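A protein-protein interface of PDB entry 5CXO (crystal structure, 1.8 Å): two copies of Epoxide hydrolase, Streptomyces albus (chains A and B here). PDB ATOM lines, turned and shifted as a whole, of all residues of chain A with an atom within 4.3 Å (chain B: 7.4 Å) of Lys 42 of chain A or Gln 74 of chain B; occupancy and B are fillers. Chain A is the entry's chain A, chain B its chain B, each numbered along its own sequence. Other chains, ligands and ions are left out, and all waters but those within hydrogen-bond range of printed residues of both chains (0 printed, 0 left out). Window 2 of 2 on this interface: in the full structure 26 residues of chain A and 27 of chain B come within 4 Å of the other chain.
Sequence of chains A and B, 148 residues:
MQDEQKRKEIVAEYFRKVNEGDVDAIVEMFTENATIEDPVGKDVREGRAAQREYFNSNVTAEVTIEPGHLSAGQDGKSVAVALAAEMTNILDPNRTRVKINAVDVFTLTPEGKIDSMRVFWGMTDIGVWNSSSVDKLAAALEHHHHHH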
ATOM      1  N   PRO A  39      -1.011 -26.326 -23.126  1.00  0.00           N
ATOM      2  CA  PRO A  39      -0.051 -26.554 -24.232  1.00  0.00           C
ATOM      3  C   PRO A  39       0.914 -27.638 -23.793  1.00  0.00           C
ATOM      4  O   PRO A  39       1.108 -27.936 -22.573  1.00  0.00           O
ATOM      5  CB  PRO A  39       0.749 -25.216 -24.281  1.00  0.00           C
ATOM      6  CG  PRO A  39       0.766 -24.786 -22.819  1.00  0.00           C
ATOM      7  CD  PRO A  39      -0.638 -25.111 -22.344  1.00  0.00           C
ATOM      8  N   VAL A  40       1.555 -28.212 -24.780  1.00  0.00           N
ATOM      9  CA  VAL A  40       2.725 -29.046 -24.544  1.00  0.00           C
ATOM     10  C   VAL A  40       3.749 -28.327 -23.668  1.00  0.00           C
ATOM     11  O   VAL A  40       4.031 -27.109 -23.865  1.00  0.00           O
ATOM     12  CB  VAL A  40       3.348 -29.454 -25.856  1.00  0.00           C
ATOM     13  CG1 VAL A  40       4.788 -29.895 -25.630  1.00  0.00           C
ATOM     14  CG2 VAL A  40       2.479 -30.522 -26.587  1.00  0.00           C
ATOM     15  N   GLY A  41       4.272 -29.081 -22.684  1.00  0.00           N
ATOM     16  CA  GLY A  41       5.144 -28.549 -21.621  1.00  0.00           C
ATOM     17  C   GLY A  41       4.499 -27.957 -20.346  1.00  0.00           C
ATOM     18  O   GLY A  41       5.200 -27.545 -19.422  1.00  0.00           O
ATOM     19  N   LYS A  42       3.197 -27.855 -20.296  1.00  0.00           N
ATOM     20  CA  LYS A  42       2.527 -27.437 -19.057  1.00  0.00           C
ATOM     21  C   LYS A  42       1.871 -28.678 -18.427  1.00  0.00           C
ATOM     22  O   LYS A  42       2.147 -29.804 -18.856  1.00  0.00           O
ATOM     23  CB  LYS A  42       1.567 -26.299 -19.350  1.00  0.00           C
ATOM     24  CG  LYS A  42       2.310 -25.000 -19.693  1.00  0.00           C
ATOM     25  CD  LYS A  42       2.117 -23.933 -18.635  1.00  0.00           C
ATOM     26  CE  LYS A  42       2.543 -22.562 -19.139  1.00  0.00           C
ATOM     27  NZ  LYS A  42       3.840 -22.149 -18.525  1.00  0.00           N
ATOM     28  N   ASP A  43       1.058 -28.499 -17.383  1.00  0.00           N
ATOM     29  CA  ASP A  43       0.472 -29.642 -16.658  1.00  0.00           C
ATOM     30  C   ASP A  43      -0.396 -30.540 -17.530  1.00  0.00           C
ATOM     31  O   ASP A  43      -1.259 -30.054 -18.231  1.00  0.00           O
ATOM     32  CB  ASP A  43      -0.345 -29.129 -15.454  1.00  0.00           C
ATOM     33  CG  ASP A  43       0.566 -28.624 -14.309  1.00  0.00           C
ATOM     34  OD1 ASP A  43       1.702 -29.121 -14.188  1.00  0.00           O
ATOM     35  OD2 ASP A  43       0.166 -27.739 -13.527  1.00  0.00           O
ATOM     36  N   VAL A  44      -0.121 -31.837 -17.513  1.00  0.00           N
ATOM     37  CA  VAL A  44      -0.988 -32.851 -18.146  1.00  0.00           C
ATOM     38  C   VAL A  44      -2.298 -33.001 -17.435  1.00  0.00           C
ATOM     39  O   VAL A  44      -2.335 -33.065 -16.200  1.00  0.00           O
ATOM     40  CB  VAL A  44      -0.253 -34.181 -18.303  1.00  0.00           C
ATOM     41  CG1 VAL A  44      -1.020 -35.146 -19.197  1.00  0.00           C
ATOM     42  CG2 VAL A  44       1.114 -33.891 -18.890  1.00  0.00           C
ATOM     43  N   TRP A 121       1.202 -25.214 -29.077  1.00  0.00           N
ATOM     44  CA  TRP A 121       1.064 -23.825 -29.452  1.00  0.00           C
ATOM     45  C   TRP A 121       1.822 -23.030 -28.438  1.00  0.00           C
ATOM     46  O   TRP A 121       1.906 -23.449 -27.278  1.00  0.00           O
ATOM     47  CB  TRP A 121      -0.397 -23.361 -29.487  1.00  0.00           C
ATOM     48  CG  TRP A 121      -1.069 -23.416 -28.044  1.00  0.00           C
ATOM     49  CD1 TRP A 121      -1.657 -24.506 -27.440  1.00  0.00           C
ATOM     50  CD2 TRP A 121      -1.097 -22.357 -27.071  1.00  0.00           C
ATOM     51  NE1 TRP A 121      -2.053 -24.185 -26.198  1.00  0.00           N
ATOM     52  CE2 TRP A 121      -1.750 -22.868 -25.931  1.00  0.00           C
ATOM     53  CE3 TRP A 121      -0.667 -21.016 -27.066  1.00  0.00           C
ATOM     54  CZ2 TRP A 121      -1.937 -22.118 -24.796  1.00  0.00           C
ATOM     55  CZ3 TRP A 121      -0.874 -20.244 -25.932  1.00  0.00           C
ATOM     56  CH2 TRP A 121      -1.530 -20.780 -24.807  1.00  0.00           C
ATOM     57  N   GLY A 122       2.425 -21.928 -28.896  1.00  0.00           N
ATOM     58  CA  GLY A 122       3.263 -21.094 -27.971  1.00  0.00           C
ATOM     59  C   GLY A 122       2.754 -19.704 -27.926  1.00  0.00           C
ATOM     60  O   GLY A 122       1.833 -19.328 -28.630  1.00  0.00           O
ATOM     61  N   GLU B   4      11.011 -19.203 -28.118  1.00  0.00           N
ATOM     62  CA  GLU B   4      10.187 -19.754 -29.237  1.00  0.00           C
ATOM     63  C   GLU B   4      10.629 -19.213 -30.610  1.00  0.00           C
ATOM     64  O   GLU B   4      10.696 -19.993 -31.543  1.00  0.00           O
ATOM     65  CB  GLU B   4       8.692 -19.429 -29.031  1.00  0.00           C
ATOM     66  CG  GLU B   4       8.051 -20.067 -27.804  1.00  0.00           C
ATOM     67  CD  GLU B   4       6.585 -19.668 -27.719  1.00  0.00           C
ATOM     68  OE1 GLU B   4       5.970 -19.704 -26.625  1.00  0.00           O
ATOM     69  OE2 GLU B   4       6.029 -19.195 -28.761  1.00  0.00           O
ATOM     70  N   ARG B   7      13.884 -20.818 -31.679  1.00  0.00           N
ATOM     71  CA  ARG B   7      13.655 -22.201 -31.928  1.00  0.00           C
ATOM     72  C   ARG B   7      13.008 -22.409 -33.324  1.00  0.00           C
ATOM     73  O   ARG B   7      13.377 -23.383 -34.042  1.00  0.00           O
ATOM     74  CB  ARG B   7      12.724 -22.744 -30.837  1.00  0.00           C
ATOM     75  CG  ARG B   7      12.611 -24.240 -30.786  1.00  0.00           C
ATOM     76  CD  ARG B   7      11.551 -24.742 -29.778  1.00  0.00           C
ATOM     77  NE  ARG B   7      11.523 -23.977 -28.523  1.00  0.00           N
ATOM     78  CZ  ARG B   7      10.477 -23.768 -27.762  1.00  0.00           C
ATOM     79  NH1 ARG B   7      10.624 -23.017 -26.695  1.00  0.00           N
ATOM     80  NH2 ARG B   7       9.275 -24.311 -28.035  1.00  0.00           N
ATOM     81  N   ALA B  72       5.106 -23.640 -31.874  1.00  0.00           N
ATOM     82  CA  ALA B  72       6.059 -23.993 -30.779  1.00  0.00           C
ATOM     83  C   ALA B  72       5.290 -24.738 -29.673  1.00  0.00           C
ATOM     84  O   ALA B  72       4.120 -24.526 -29.472  1.00  0.00           O
ATOM     85  CB  ALA B  72       6.618 -22.717 -30.206  1.00  0.00           C
ATOM     86  N   GLY B  73       5.955 -25.685 -29.077  1.00  0.00           N
ATOM     87  CA  GLY B  73       5.587 -26.241 -27.749  1.00  0.00           C
ATOM     88  C   GLY B  73       6.002 -25.239 -26.669  1.00  0.00           C
ATOM     89  O   GLY B  73       6.820 -24.301 -26.890  1.00  0.00           O
ATOM     90  N   GLN B  74       5.421 -25.380 -25.474  1.00  0.00           N
ATOM     91  CA  GLN B  74       5.797 -24.435 -24.336  1.00  0.00           C
ATOM     92  C   GLN B  74       6.617 -25.272 -23.352  1.00  0.00           C
ATOM     93  O   GLN B  74       6.571 -25.110 -22.112  1.00  0.00           O
ATOM     94  CB  GLN B  74       4.542 -23.876 -23.664  1.00  0.00           C
ATOM     95  CG  GLN B  74       3.907 -22.808 -24.561  1.00  0.00           C
ATOM     96  CD  GLN B  74       2.726 -22.101 -23.982  1.00  0.00           C
ATOM     97  OE1 GLN B  74       2.840 -21.497 -22.883  1.00  0.00           O
ATOM     98  NE2 GLN B  74       1.567 -22.053 -24.740  1.00  0.00           N
ATOM     99  N   ASP B  75       7.423 -26.123 -23.934  1.00  0.00           N
ATOM    100  CA  ASP B  75       8.258 -27.031 -23.186  1.00  0.00           C
ATOM    101  C   ASP B  75       9.739 -26.708 -23.290  1.00  0.00           C
ATOM    102  O   ASP B  75      10.572 -27.569 -22.989  1.00  0.00           O
ATOM    103  CB  ASP B  75       7.909 -28.443 -23.663  1.00  0.00           C
ATOM    104  CG  ASP B  75       8.295 -28.682 -25.167  1.00  0.00           C
ATOM    105  OD1 ASP B  75       8.249 -29.853 -25.618  1.00  0.00           O
ATOM    106  OD2 ASP B  75       8.668 -27.691 -25.848  1.00  0.00           O
ATOM    107  N   GLY B  76      10.057 -25.506 -23.814  1.00  0.00           N
ATOM    108  CA  GLY B  76      11.369 -25.056 -24.026  1.00  0.00           C
ATOM    109  C   GLY B  76      12.141 -25.746 -25.104  1.00  0.00           C
ATOM    110  O   GLY B  76      13.348 -25.453 -25.263  1.00  0.00           O
ATOM    111  N   LYS B  77      11.477 -26.590 -25.900  1.00  0.00           N
ATOM    112  CA  LYS B  77      12.214 -27.223 -26.975  1.00  0.00           C
ATOM    113  C   LYS B  77      11.481 -27.746 -28.247  1.00  0.00           C
ATOM    114  O   LYS B  77      12.131 -28.229 -29.168  1.00  0.00           O
ATOM    115  CB  LYS B  77      13.003 -28.374 -26.380  1.00  0.00           C
ATOM    116  CG  LYS B  77      12.170 -29.569 -26.148  1.00  0.00           C
ATOM    117  CD  LYS B  77      13.073 -30.652 -25.545  1.00  0.00           C
ATOM    118  CE  LYS B  77      12.182 -31.710 -24.950  1.00  0.00           C
ATOM    119  NZ  LYS B  77      11.173 -30.958 -24.177  1.00  0.00           N
ATOM    120  N   SER B  78      10.163 -27.794 -28.255  1.00  0.00           N
ATOM    121  CA  SER B  78       9.479 -28.443 -29.423  1.00  0.00           C
ATOM    122  C   SER B  78       8.997 -27.437 -30.469  1.00  0.00           C
ATOM    123  O   SER B  78       8.616 -26.321 -30.125  1.00  0.00           O
ATOM    124  CB  SER B  78       8.256 -29.206 -28.910  1.00  0.00           C
ATOM    125  OG  SER B  78       8.620 -30.343 -28.126  1.00  0.00           O
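The backbone carbonyl oxygen (O) of Val 40 of chain A sits at hydrogen-bond distance from the backbone NH (N) of Gln 74 of chain B (2.7 Å). The backbone NH (N) of Trp 121 of chain A lies close to the backbone carbonyl oxygen (O) of Ala 72 of chain B. The backbone carbonyl oxygen (O) of Trp 121 of chain A sits at hydrogen-bond distance from the side-chain amide nitrogen (NE2) of Gln 74 of chain B (2.9 Å). N of Gly 122 of chain A is in hydrogen-bond range of O of Ala 72 of chain B (3.2 Å).
NH2 of Arg 7 of chain B lies within hydrogen-bond range of O of Gly 73 of chain B, 2.7 Å away. The backbone NH (N) of Gly 73 of chain B lies within hydrogen-bond range of the backbone carbonyl oxygen (O) of Ser 78 of chain B (2.9 Å). The side-chain amino group (NZ) of Lys 77 of chain B is in salt-bridge range of the side-chain carboxylate (OD1) of Asp 75 of chain B, at 3.4 Å. The side-chain carboxylate of Asp 75 of chain B lies within hydrogen-bond range of the side-chain hydroxyl of Ser 78 of chain B.
Gln 74 of chain B touches Pro 39 of chain A. Val 40 of chain A touches Gly 73 of chain B (O to C, 3.9 Å). Val 40 of chain A touches Asp 75 of chain B. Gly 41 of chain A touches Gln 74 of chain B (CA to O, 3.8 Å). Asp 75 of chain B touches Gly 41 of chain A (CB to CA, 3.4 Å). Gln 74 of chain B touches Lys 42 of chain A. Glu 4 of chain B touches Gly 122 of chain A. Gln 74 of chain B touches Gly 122 of chain A.
Of the printed residues of chain B, Val 40 of chain A touches Gly 73 (3.9 Å), Gln 74 (2.7 Å) and Asp 75 (3.5 Å). Of chain B, only Gln 74 and Asp 75 come within 4 Å of Gly 41 of chain A. Of chain B, only Gln 74 (3.9 Å) comes within 4 Å of Lys 42 of chain A. Asp 43 of chain A touches none of the printed residues of chain B. Val 44 of chain A touches none of the printed residues of chain B. Of the printed residues of chain B, Trp 121 of chain A touches Ala 72 (2.9 Å) and Gln 74 (2.9 Å). Of the printed residues of chain B, Gly 122 of chain A touches Glu 4, Ala 72 and Gln 74. Of the printed residues of chain A, Glu 4 of chain B touches Gly 122 (3.3 Å). Printed residues of chain A within 4 Å of Ala 72 of chain B: Trp 121 (2.9 Å) and Gly 122 (3.2 Å). Of chain A, only Pro 39, Val 40, Gly 41, Lys 42, Trp 121 and Gly 122 come within 4 Å of Gln 74 of chain B.
Of the 9 printed residues of chain B, 5 touch a printed residue of chain A.
No position is printed for both chains. Of the 12 pairs that touch across the chains among the printed residues, none has its exchanged pair printed and touching as well.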
